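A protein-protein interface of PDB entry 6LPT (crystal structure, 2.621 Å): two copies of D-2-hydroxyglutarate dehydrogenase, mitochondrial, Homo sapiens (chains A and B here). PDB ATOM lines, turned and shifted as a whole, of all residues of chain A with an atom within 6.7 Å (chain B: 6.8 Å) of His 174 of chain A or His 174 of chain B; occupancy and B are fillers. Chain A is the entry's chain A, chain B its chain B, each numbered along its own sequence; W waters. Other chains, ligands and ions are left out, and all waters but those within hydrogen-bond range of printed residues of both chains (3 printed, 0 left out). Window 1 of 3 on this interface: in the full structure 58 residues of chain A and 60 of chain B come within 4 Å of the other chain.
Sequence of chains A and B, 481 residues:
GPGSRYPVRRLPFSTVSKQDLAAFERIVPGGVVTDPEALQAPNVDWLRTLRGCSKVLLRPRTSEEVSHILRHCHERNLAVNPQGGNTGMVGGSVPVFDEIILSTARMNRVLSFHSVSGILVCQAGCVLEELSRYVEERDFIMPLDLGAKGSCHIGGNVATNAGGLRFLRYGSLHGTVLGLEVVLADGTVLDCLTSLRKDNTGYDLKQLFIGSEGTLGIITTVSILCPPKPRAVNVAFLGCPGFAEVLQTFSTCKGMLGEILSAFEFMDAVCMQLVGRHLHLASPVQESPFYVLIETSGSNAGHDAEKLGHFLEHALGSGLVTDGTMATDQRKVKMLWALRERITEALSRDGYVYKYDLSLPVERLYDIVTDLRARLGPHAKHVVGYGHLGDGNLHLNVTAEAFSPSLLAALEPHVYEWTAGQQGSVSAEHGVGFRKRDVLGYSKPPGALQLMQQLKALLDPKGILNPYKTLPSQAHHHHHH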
ATOM      1  N   ASN A 161      -5.726 -28.301 -20.377  1.00  0.00           N
ATOM      2  CA  ASN A 161      -6.066 -27.651 -19.110  1.00  0.00           C
ATOM      3  C   ASN A 161      -5.633 -28.525 -17.933  1.00  0.00           C
ATOM      4  O   ASN A 161      -6.432 -28.949 -17.095  1.00  0.00           O
ATOM      5  CB  ASN A 161      -7.559 -27.313 -19.034  1.00  0.00           C
ATOM      6  CG  ASN A 161      -7.922 -26.550 -17.766  1.00  0.00           C
ATOM      7  OD1 ASN A 161      -7.154 -25.712 -17.290  1.00  0.00           O
ATOM      8  ND2 ASN A 161      -9.088 -26.856 -17.204  1.00  0.00           N
ATOM      9  N   GLY A 171      -4.259 -22.963  -8.528  1.00  0.00           N
ATOM     10  CA  GLY A 171      -5.467 -23.000  -9.323  1.00  0.00           C
ATOM     11  C   GLY A 171      -5.235 -23.247 -10.805  1.00  0.00           C
ATOM     12  O   GLY A 171      -4.188 -23.730 -11.247  1.00  0.00           O
ATOM     13  N   SER A 172      -6.260 -22.904 -11.580  1.00  0.00           N
ATOM     14  CA  SER A 172      -6.388 -23.352 -12.959  1.00  0.00           C
ATOM     15  C   SER A 172      -5.508 -22.543 -13.904  1.00  0.00           C
ATOM     16  O   SER A 172      -5.180 -21.381 -13.651  1.00  0.00           O
ATOM     17  CB  SER A 172      -7.845 -23.263 -13.410  1.00  0.00           C
ATOM     18  OG  SER A 172      -7.980 -23.614 -14.775  1.00  0.00           O
ATOM     19  N   LEU A 173      -5.115 -23.186 -15.007  1.00  0.00           N
ATOM     20  CA  LEU A 173      -4.508 -22.458 -16.114  1.00  0.00           C
ATOM     21  C   LEU A 173      -5.455 -21.402 -16.674  1.00  0.00           C
ATOM     22  O   LEU A 173      -5.001 -20.395 -17.226  1.00  0.00           O
ATOM     23  CB  LEU A 173      -4.084 -23.436 -17.210  1.00  0.00           C
ATOM     24  CG  LEU A 173      -2.918 -24.367 -16.864  1.00  0.00           C
ATOM     25  CD1 LEU A 173      -2.791 -25.480 -17.892  1.00  0.00           C
ATOM     26  CD2 LEU A 173      -1.616 -23.588 -16.750  1.00  0.00           C
ATOM     27  N   HIS A 174      -6.768 -21.612 -16.546  1.00  0.00           N
ATOM     28  CA  HIS A 174      -7.730 -20.571 -16.900  1.00  0.00           C
ATOM     29  C   HIS A 174      -7.478 -19.275 -16.137  1.00  0.00           C
ATOM     30  O   HIS A 174      -7.814 -18.191 -16.629  1.00  0.00           O
ATOM     31  CB  HIS A 174      -9.161 -21.054 -16.647  1.00  0.00           C
ATOM     32  CG  HIS A 174      -9.624 -22.115 -17.599  1.00  0.00           C
ATOM     33  ND1 HIS A 174      -9.903 -21.854 -18.923  1.00  0.00           N
ATOM     34  CD2 HIS A 174      -9.872 -23.433 -17.415  1.00  0.00           C
ATOM     35  CE1 HIS A 174     -10.294 -22.968 -19.516  1.00  0.00           C
ATOM     36  NE2 HIS A 174     -10.286 -23.941 -18.624  1.00  0.00           N
ATOM     37  N   GLY A 175      -6.896 -19.360 -14.943  1.00  0.00           N
ATOM     38  CA  GLY A 175      -6.496 -18.178 -14.209  1.00  0.00           C
ATOM     39  C   GLY A 175      -5.053 -17.762 -14.403  1.00  0.00           C
ATOM     40  O   GLY A 175      -4.752 -16.565 -14.423  1.00  0.00           O
ATOM     41  N   THR A 176      -4.149 -18.730 -14.549  1.00  0.00           N
ATOM     42  CA  THR A 176      -2.724 -18.425 -14.576  1.00  0.00           C
ATOM     43  C   THR A 176      -2.185 -18.142 -15.971  1.00  0.00           C
ATOM     44  O   THR A 176      -1.141 -17.493 -16.093  1.00  0.00           O
ATOM     45  CB  THR A 176      -1.923 -19.579 -13.963  1.00  0.00           C
ATOM     46  OG1 THR A 176      -2.179 -20.785 -14.695  1.00  0.00           O
ATOM     47  CG2 THR A 176      -2.318 -19.789 -12.513  1.00  0.00           C
ATOM     48  N   VAL A 177      -2.861 -18.594 -17.021  1.00  0.00           N
ATOM     49  CA  VAL A 177      -2.436 -18.266 -18.377  1.00  0.00           C
ATOM     50  C   VAL A 177      -2.859 -16.834 -18.676  1.00  0.00           C
ATOM     51  O   VAL A 177      -4.039 -16.486 -18.564  1.00  0.00           O
ATOM     52  CB  VAL A 177      -3.024 -19.244 -19.403  1.00  0.00           C
ATOM     53  CG1 VAL A 177      -2.767 -18.745 -20.818  1.00  0.00           C
ATOM     54  CG2 VAL A 177      -2.427 -20.629 -19.216  1.00  0.00           C
ATOM     55  N   ASN A 200      -9.465  -6.406 -19.656  1.00  0.00           N
ATOM     56  CA  ASN A 200     -10.869  -6.615 -20.024  1.00  0.00           C
ATOM     57  C   ASN A 200     -11.249  -5.832 -21.277  1.00  0.00           C
ATOM     58  O   ASN A 200     -12.244  -5.105 -21.285  1.00  0.00           O
ATOM     59  CB  ASN A 200     -11.784  -6.251 -18.859  1.00  0.00           C
ATOM     60  CG  ASN A 200     -11.853  -7.340 -17.804  1.00  0.00           C
ATOM     61  OD1 ASN A 200     -11.311  -8.430 -17.984  1.00  0.00           O
ATOM     62  ND2 ASN A 200     -12.532  -7.052 -16.699  1.00  0.00           N
ATOM     63  N   ASP A 204     -12.466 -12.904 -23.824  1.00  0.00           N
ATOM     64  CA  ASP A 204     -11.242 -13.594 -23.417  1.00  0.00           C
ATOM     65  C   ASP A 204     -11.057 -14.815 -24.321  1.00  0.00           C
ATOM     66  O   ASP A 204     -11.230 -15.968 -23.920  1.00  0.00           O
ATOM     67  CB  ASP A 204     -11.310 -13.969 -21.942  1.00  0.00           C
ATOM     68  CG  ASP A 204      -9.946 -14.266 -21.347  1.00  0.00           C
ATOM     69  OD1 ASP A 204      -8.952 -14.274 -22.103  1.00  0.00           O
ATOM     70  OD2 ASP A 204      -9.871 -14.485 -20.117  1.00  0.00           O
ATOM     71  N   LYS A 206      -8.609 -16.409 -25.562  1.00  0.00           N
ATOM     72  CA  LYS A 206      -7.638 -17.447 -25.229  1.00  0.00           C
ATOM     73  C   LYS A 206      -8.289 -18.582 -24.453  1.00  0.00           C
ATOM     74  O   LYS A 206      -7.865 -19.738 -24.571  1.00  0.00           O
ATOM     75  CB  LYS A 206      -6.469 -16.843 -24.447  1.00  0.00           C
ATOM     76  CG  LYS A 206      -6.800 -16.480 -23.012  1.00  0.00           C
ATOM     77  CD  LYS A 206      -5.626 -15.842 -22.308  1.00  0.00           C
ATOM     78  CE  LYS A 206      -5.965 -15.576 -20.858  1.00  0.00           C
ATOM     79  NZ  LYS A 206      -6.744 -14.320 -20.694  1.00  0.00           N
ATOM     80  N   GLN A 207      -9.314 -18.269 -23.658  1.00  0.00           N
ATOM     81  CA  GLN A 207      -9.997 -19.277 -22.857  1.00  0.00           C
ATOM     82  C   GLN A 207     -10.534 -20.420 -23.715  1.00  0.00           C
ATOM     83  O   GLN A 207     -10.576 -21.567 -23.256  1.00  0.00           O
ATOM     84  CB  GLN A 207     -11.126 -18.623 -22.066  1.00  0.00           C
ATOM     85  CG  GLN A 207     -10.662 -17.602 -21.035  1.00  0.00           C
ATOM     86  CD  GLN A 207      -9.925 -18.221 -19.864  1.00  0.00           C
ATOM     87  OE1 GLN A 207      -9.847 -19.442 -19.733  1.00  0.00           O
ATOM     88  NE2 GLN A 207      -9.374 -17.374 -19.002  1.00  0.00           N
ATOM     89  N   LEU A 208     -10.966 -20.130 -24.951  1.00  0.00           N
ATOM     90  CA  LEU A 208     -11.421 -21.196 -25.843  1.00  0.00           C
ATOM     91  C   LEU A 208     -10.355 -22.248 -26.099  1.00  0.00           C
ATOM     92  O   LEU A 208     -10.681 -23.423 -26.292  1.00  0.00           O
ATOM     93  CB  LEU A 208     -11.856 -20.618 -27.191  1.00  0.00           C
ATOM     94  CG  LEU A 208     -13.149 -19.844 -27.343  1.00  0.00           C
ATOM     95  CD1 LEU A 208     -13.290 -19.348 -28.756  1.00  0.00           C
ATOM     96  CD2 LEU A 208     -14.202 -20.895 -27.129  1.00  0.00           C
ATOM     97  N   PHE A 209      -9.090 -21.862 -26.097  1.00  0.00           N
ATOM     98  CA  PHE A 209      -8.043 -22.801 -26.461  1.00  0.00           C
ATOM     99  C   PHE A 209      -7.451 -23.526 -25.262  1.00  0.00           C
ATOM    100  O   PHE A 209      -6.668 -24.463 -25.448  1.00  0.00           O
ATOM    101  CB  PHE A 209      -6.974 -22.065 -27.266  1.00  0.00           C
ATOM    102  CG  PHE A 209      -7.526 -21.417 -28.503  1.00  0.00           C
ATOM    103  CD1 PHE A 209      -7.678 -22.140 -29.676  1.00  0.00           C
ATOM    104  CD2 PHE A 209      -7.951 -20.099 -28.475  1.00  0.00           C
ATOM    105  CE1 PHE A 209      -8.213 -21.549 -30.808  1.00  0.00           C
ATOM    106  CE2 PHE A 209      -8.485 -19.504 -29.598  1.00  0.00           C
ATOM    107  CZ  PHE A 209      -8.616 -20.229 -30.769  1.00  0.00           C
ATOM    108  N   ILE A 210      -7.810 -23.126 -24.048  1.00  0.00           N
ATOM    109  CA  ILE A 210      -7.350 -23.802 -22.842  1.00  0.00           C
ATOM    110  C   ILE A 210      -8.335 -24.933 -22.572  1.00  0.00           C
ATOM    111  O   ILE A 210      -9.499 -24.690 -22.246  1.00  0.00           O
ATOM    112  CB  ILE A 210      -7.274 -22.835 -21.655  1.00  0.00           C
ATOM    113  CG1 ILE A 210      -6.365 -21.649 -21.982  1.00  0.00           C
ATOM    114  CG2 ILE A 210      -6.784 -23.557 -20.406  1.00  0.00           C
ATOM    115  CD1 ILE A 210      -6.418 -20.538 -20.953  1.00  0.00           C
ATOM    116  N   GLY A 211      -7.870 -26.170 -22.710  1.00  0.00           N
ATOM    117  CA  GLY A 211      -8.747 -27.317 -22.644  1.00  0.00           C
ATOM    118  C   GLY A 211      -9.370 -27.741 -23.956  1.00  0.00           C
ATOM    119  O   GLY A 211     -10.216 -28.643 -23.953  1.00  0.00           O
ATOM    120  N   VAL B 158     -19.716 -11.227 -12.955  1.00  0.00           N
ATOM    121  CA  VAL B 158     -19.270 -12.227 -13.922  1.00  0.00           C
ATOM    122  C   VAL B 158     -19.272 -11.663 -15.341  1.00  0.00           C
ATOM    123  O   VAL B 158     -18.323 -11.876 -16.106  1.00  0.00           O
ATOM    124  CB  VAL B 158     -20.130 -13.502 -13.819  1.00  0.00           C
ATOM    125  CG1 VAL B 158     -19.720 -14.501 -14.895  1.00  0.00           C
ATOM    126  CG2 VAL B 158     -20.002 -14.120 -12.435  1.00  0.00           C
ATOM    127  N   ASN B 161     -16.378  -9.418 -15.734  1.00  0.00           N
ATOM    128  CA  ASN B 161     -15.131  -9.982 -15.208  1.00  0.00           C
ATOM    129  C   ASN B 161     -14.478  -9.033 -14.200  1.00  0.00           C
ATOM    130  O   ASN B 161     -13.320  -8.630 -14.337  1.00  0.00           O
ATOM    131  CB  ASN B 161     -14.173 -10.346 -16.347  1.00  0.00           C
ATOM    132  CG  ASN B 161     -12.902 -11.001 -15.851  1.00  0.00           C
ATOM    133  OD1 ASN B 161     -12.923 -11.760 -14.882  1.00  0.00           O
ATOM    134  ND2 ASN B 161     -11.786 -10.711 -16.512  1.00  0.00           N
ATOM    135  N   GLY B 171      -7.446 -14.041  -7.240  1.00  0.00           N
ATOM    136  CA  GLY B 171      -7.394 -14.122  -8.689  1.00  0.00           C
ATOM    137  C   GLY B 171      -8.703 -13.850  -9.415  1.00  0.00           C
ATOM    138  O   GLY B 171      -9.701 -13.387  -8.854  1.00  0.00           O
ATOM    139  N   SER B 172      -8.674 -14.166 -10.710  1.00  0.00           N
ATOM    140  CA  SER B 172      -9.759 -13.835 -11.625  1.00  0.00           C
ATOM    141  C   SER B 172     -11.001 -14.693 -11.405  1.00  0.00           C
ATOM    142  O   SER B 172     -10.933 -15.826 -10.921  1.00  0.00           O
ATOM    143  CB  SER B 172      -9.287 -13.994 -13.072  1.00  0.00           C
ATOM    144  OG  SER B 172     -10.345 -13.783 -13.990  1.00  0.00           O
ATOM    145  N   LEU B 173     -12.153 -14.121 -11.775  1.00  0.00           N
ATOM    146  CA  LEU B 173     -13.388 -14.888 -11.895  1.00  0.00           C
ATOM    147  C   LEU B 173     -13.270 -16.000 -12.928  1.00  0.00           C
ATOM    148  O   LEU B 173     -13.965 -17.018 -12.828  1.00  0.00           O
ATOM    149  CB  LEU B 173     -14.550 -13.960 -12.246  1.00  0.00           C
ATOM    150  CG  LEU B 173     -14.983 -13.004 -11.134  1.00  0.00           C
ATOM    151  CD1 LEU B 173     -15.994 -11.998 -11.654  1.00  0.00           C
ATOM    152  CD2 LEU B 173     -15.551 -13.789  -9.963  1.00  0.00           C
ATOM    153  N   HIS B 174     -12.412 -15.817 -13.935  1.00  0.00           N
ATOM    154  CA  HIS B 174     -12.121 -16.897 -14.872  1.00  0.00           C
ATOM    155  C   HIS B 174     -11.599 -18.137 -14.155  1.00  0.00           C
ATOM    156  O   HIS B 174     -11.743 -19.255 -14.665  1.00  0.00           O
ATOM    157  CB  HIS B 174     -11.107 -16.419 -15.917  1.00  0.00           C
ATOM    158  CG  HIS B 174     -11.653 -15.406 -16.879  1.00  0.00           C
ATOM    159  ND1 HIS B 174     -12.513 -15.733 -17.905  1.00  0.00           N
ATOM    160  CD2 HIS B 174     -11.467 -14.068 -16.959  1.00  0.00           C
ATOM    161  CE1 HIS B 174     -12.825 -14.642 -18.582  1.00  0.00           C
ATOM    162  NE2 HIS B 174     -12.205 -13.616 -18.026  1.00  0.00           N
ATOM    163  N   GLY B 175     -10.989 -17.964 -12.983  1.00  0.00           N
ATOM    164  CA  GLY B 175     -10.598 -19.074 -12.137  1.00  0.00           C
ATOM    165  C   GLY B 175     -11.590 -19.486 -11.068  1.00  0.00           C
ATOM    166  O   GLY B 175     -11.727 -20.678 -10.781  1.00  0.00           O
ATOM    167  N   THR B 176     -12.294 -18.520 -10.471  1.00  0.00           N
ATOM    168  CA  THR B 176     -13.131 -18.809  -9.312  1.00  0.00           C
ATOM    169  C   THR B 176     -14.570 -19.162  -9.665  1.00  0.00           C
ATOM    170  O   THR B 176     -15.250 -19.799  -8.851  1.00  0.00           O
ATOM    171  CB  THR B 176     -13.136 -17.621  -8.346  1.00  0.00           C
ATOM    172  OG1 THR B 176     -13.493 -16.427  -9.053  1.00  0.00           O
ATOM    173  CG2 THR B 176     -11.761 -17.440  -7.713  1.00  0.00           C
ATOM    174  N   VAL B 177     -15.053 -18.777 -10.844  1.00  0.00           N
ATOM    175  CA  VAL B 177     -16.374 -19.213 -11.281  1.00  0.00           C
ATOM    176  C   VAL B 177     -16.292 -20.676 -11.690  1.00  0.00           C
ATOM    177  O   VAL B 177     -15.514 -21.047 -12.576  1.00  0.00           O
ATOM    178  CB  VAL B 177     -16.898 -18.341 -12.427  1.00  0.00           C
ATOM    179  CG1 VAL B 177     -18.188 -18.922 -12.979  1.00  0.00           C
ATOM    180  CG2 VAL B 177     -17.114 -16.914 -11.945  1.00  0.00           C
ATOM    181  N   ASN B 200     -12.899 -31.450 -16.915  1.00  0.00           N
ATOM    182  CA  ASN B 200     -12.391 -31.294 -18.280  1.00  0.00           C
ATOM    183  C   ASN B 200     -13.174 -32.164 -19.264  1.00  0.00           C
ATOM    184  O   ASN B 200     -12.607 -32.972 -19.997  1.00  0.00           O
ATOM    185  CB  ASN B 200     -10.900 -31.630 -18.335  1.00  0.00           C
ATOM    186  CG  ASN B 200     -10.022 -30.496 -17.836  1.00  0.00           C
ATOM    187  OD1 ASN B 200     -10.495 -29.382 -17.624  1.00  0.00           O
ATOM    188  ND2 ASN B 200      -8.736 -30.779 -17.646  1.00  0.00           N
ATOM    189  N   ASP B 204     -14.626 -25.336 -22.247  1.00  0.00           N
ATOM    190  CA  ASP B 204     -15.033 -24.566 -21.070  1.00  0.00           C
ATOM    191  C   ASP B 204     -15.893 -23.396 -21.553  1.00  0.00           C
ATOM    192  O   ASP B 204     -15.475 -22.237 -21.587  1.00  0.00           O
ATOM    193  CB  ASP B 204     -13.824 -24.098 -20.271  1.00  0.00           C
ATOM    194  CG  ASP B 204     -14.174 -23.762 -18.832  1.00  0.00           C
ATOM    195  OD1 ASP B 204     -15.358 -23.922 -18.461  1.00  0.00           O
ATOM    196  OD2 ASP B 204     -13.266 -23.341 -18.078  1.00  0.00           O
ATOM    197  N   LYS B 206     -18.380 -21.750 -20.414  1.00  0.00           N
ATOM    198  CA  LYS B 206     -18.700 -20.651 -19.510  1.00  0.00           C
ATOM    199  C   LYS B 206     -17.698 -19.507 -19.612  1.00  0.00           C
ATOM    200  O   LYS B 206     -18.068 -18.344 -19.409  1.00  0.00           O
ATOM    201  CB  LYS B 206     -18.774 -21.164 -18.071  1.00  0.00           C
ATOM    202  CG  LYS B 206     -17.428 -21.515 -17.476  1.00  0.00           C
ATOM    203  CD  LYS B 206     -17.550 -21.940 -16.030  1.00  0.00           C
ATOM    204  CE  LYS B 206     -16.186 -22.271 -15.456  1.00  0.00           C
ATOM    205  NZ  LYS B 206     -15.756 -23.649 -15.812  1.00  0.00           N
ATOM    206  N   GLN B 207     -16.440 -19.807 -19.951  1.00  0.00           N
ATOM    207  CA  GLN B 207     -15.434 -18.754 -20.031  1.00  0.00           C
ATOM    208  C   GLN B 207     -15.819 -17.674 -21.032  1.00  0.00           C
ATOM    209  O   GLN B 207     -15.484 -16.499 -20.836  1.00  0.00           O
ATOM    210  CB  GLN B 207     -14.083 -19.353 -20.428  1.00  0.00           C
ATOM    211  CG  GLN B 207     -13.441 -20.324 -19.440  1.00  0.00           C
ATOM    212  CD  GLN B 207     -13.127 -19.695 -18.091  1.00  0.00           C
ATOM    213  OE1 GLN B 207     -13.035 -18.473 -17.964  1.00  0.00           O
ATOM    214  NE2 GLN B 207     -12.941 -20.535 -17.079  1.00  0.00           N
ATOM    215  N   LEU B 208     -16.505 -18.050 -22.116  1.00  0.00           N
ATOM    216  CA  LEU B 208     -16.934 -17.052 -23.095  1.00  0.00           C
ATOM    217  C   LEU B 208     -17.852 -16.001 -22.493  1.00  0.00           C
ATOM    218  O   LEU B 208     -17.836 -14.849 -22.931  1.00  0.00           O
ATOM    219  CB  LEU B 208     -17.599 -17.705 -24.308  1.00  0.00           C
ATOM    220  CG  LEU B 208     -16.734 -18.499 -25.297  1.00  0.00           C
ATOM    221  CD1 LEU B 208     -15.688 -19.353 -24.609  1.00  0.00           C
ATOM    222  CD2 LEU B 208     -17.602 -19.356 -26.210  1.00  0.00           C
ATOM    223  N   PHE B 209     -18.640 -16.364 -21.486  1.00  0.00           N
ATOM    224  CA  PHE B 209     -19.612 -15.437 -20.930  1.00  0.00           C
ATOM    225  C   PHE B 209     -19.054 -14.616 -19.780  1.00  0.00           C
ATOM    226  O   PHE B 209     -19.706 -13.664 -19.341  1.00  0.00           O
ATOM    227  CB  PHE B 209     -20.852 -16.213 -20.486  1.00  0.00           C
ATOM    228  CG  PHE B 209     -21.453 -17.038 -21.585  1.00  0.00           C
ATOM    229  CD1 PHE B 209     -22.287 -16.462 -22.527  1.00  0.00           C
ATOM    230  CD2 PHE B 209     -21.143 -18.383 -21.705  1.00  0.00           C
ATOM    231  CE1 PHE B 209     -22.824 -17.216 -23.550  1.00  0.00           C
ATOM    232  CE2 PHE B 209     -21.677 -19.142 -22.726  1.00  0.00           C
ATOM    233  CZ  PHE B 209     -22.521 -18.559 -23.649  1.00  0.00           C
ATOM    234  N   ILE B 210     -17.868 -14.965 -19.293  1.00  0.00           N
ATOM    235  CA  ILE B 210     -17.179 -14.189 -18.269  1.00  0.00           C
ATOM    236  C   ILE B 210     -16.455 -13.065 -19.004  1.00  0.00           C
ATOM    237  O   ILE B 210     -15.538 -13.316 -19.790  1.00  0.00           O
ATOM    238  CB  ILE B 210     -16.211 -15.059 -17.461  1.00  0.00           C
ATOM    239  CG1 ILE B 210     -16.975 -16.223 -16.822  1.00  0.00           C
ATOM    240  CG2 ILE B 210     -15.516 -14.225 -16.397  1.00  0.00           C
ATOM    241  CD1 ILE B 210     -16.115 -17.179 -16.036  1.00  0.00           C
ATOM    242  N   GLY B 211     -16.863 -11.824 -18.753  1.00  0.00           N
ATOM    243  CA  GLY B 211     -16.296 -10.692 -19.455  1.00  0.00           C
ATOM    244  C   GLY B 211     -16.961 -10.337 -20.772  1.00  0.00           C
ATOM    245  O   GLY B 211     -16.457  -9.456 -21.479  1.00  0.00           O
HETATM  246  O   HOH W   1      -6.471 -15.282 -11.753  1.00  0.00           O
HETATM  247  O   HOH W   2     -15.164 -13.516 -22.829  1.00  0.00           O
HETATM  248  O   HOH W   3     -11.868 -24.993 -23.539  1.00  0.00           O
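OD1 of Asn 200 of chain B lies within hydrogen-bond range of ND2 of Asn 161 of chain A, 2.9 Å away. The side-chain carboxylate of Asp 204 of chain B sits at hydrogen-bond distance from a ring nitrogen (NE2) of His 174 of chain A (3.1 Å). The side-chain amide oxygen (OD1) of Asn 200 of chain A is in hydrogen-bond range of the side-chain amide nitrogen (ND2) of Asn 161 of chain B (2.8 Å). The side-chain carboxylate (OD2) of Asp 204 of chain A lies within hydrogen-bond range of a ring nitrogen (NE2) of His 174 of chain B (3.3 Å).
Water W1 bridges the backbone NH of Ser 172 of chain B (2.7 Å) and the backbone carbonyl oxygen of Gly 175 of chain A (3.4 Å). Water W3 lies within hydrogen-bond range of the backbone carbonyl oxygen (O) of Ile 210 of chain A (2.7 Å), the backbone NH (N) of Asp 204 of chain B (3.1 Å) and the backbone carbonyl oxygen (O) of Leu 208 of chain A (3.4 Å). Water W2 lies within hydrogen-bond range of the backbone NH of Asp 204 of chain A (2.9 Å), the backbone carbonyl oxygen of Leu 208 of chain B (3.0 Å) and the backbone carbonyl oxygen of Ile 210 of chain B (3.1 Å).
His 174 of chain B touches just these residues of chain A: His 174 (3.7 Å), Asp 204 (3.3 Å) and Gln 207 (3.7 Å). Printed residues of chain A within 4 Å of Asn 161 of chain B: Asn 200 (2.8 Å). Of the printed residues of chain B, Asp 204 of chain A touches His 174. Printed residues of chain B within 4 Å of Asn 161 of chain A: Asn 200 (2.9 Å). Gly 171 of chain A touches none of the printed residues of chain B. Gly 175 of chain A touches none of the printed residues of chain B. The nearest residue of chain B that does not touch His 174 of chain A is Gly 175 of chain B (4.8 Å). The nearest residue of chain A that does not touch His 174 of chain B is Gly 175 of chain A (4.9 Å).
OG of Ser 172 of chain A lies within hydrogen-bond range of OD1 of Asn 161 of chain A, at 3.4 Å. A ring nitrogen (ND1) of His 174 of chain A lies within hydrogen-bond range of the side-chain amide oxygen of Gln 207 of chain A. ND2 of Asn 161 of chain B lies within hydrogen-bond range of NE2 of His 174 of chain B (3.3 Å). OG of Ser 172 of chain B sits at hydrogen-bond distance from N of His 174 of chain B. A ring nitrogen (ND1) of His 174 of chain B is in hydrogen-bond range of the side-chain amide oxygen (OE1) of Gln 207 of chain B (2.8 Å). The side-chain carboxylate of Asp 204 of chain B is in salt-bridge range of the side-chain amino group of Lys 206 of chain B, 2.7 Å away.
Asn 161 of chain A touches Asn 200 of chain B, and with the chains exchanged Asn 200 of chain A touches Asn 161 of chain B. His 174 of chain A touches its own counterpart, His 174 of chain B. His 174 of chain A touches Asp 204 of chain B, and with the chains exchanged Asp 204 of chain A touches His 174 of chain B. Leu 208 of chain B touches its own counterpart, Leu 208 of chain A. Positions printed for both chains: 161, 171, 172, 173, 174, 175, 176, 177, 200, 204, 206, 207, 208, 209, 210 and 211.
CB of His 174 of chain A touches O of His 174 of chain B, 3.7 Å away. His 174 of chain A touches Gln 207 of chain B (CG to NE2, 3.7 Å). CB of His 174 of chain B touches NE2 of Gln 207 of chain A (3.7 Å). CB of Gln 207 of chain B touches CB of Gln 207 of chain A, at 3.5 Å. Leu 208 of chain A touches Leu 208 of chain B (CD2 to CD1, 3.3 Å).
Of the 17 printed residues of chain B, 6 touch a printed residue of chain A. Hydrophobic or aromatic side chains of chain B that line the printed part of chain A: His 174 and Leu 208. Of the 16 printed residues of chain A, 6 touch a printed residue of chain B. Hydrophobic or aromatic side chains of chain A that line the printed part of chain B: His 174 and Leu 208. Among the printed residues, 9 pairs touch across the chains. Among the printed residues, no Asp or Glu carboxylate lies within 4 Å of a Lys or Arg side-chain nitrogen of the other chain.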
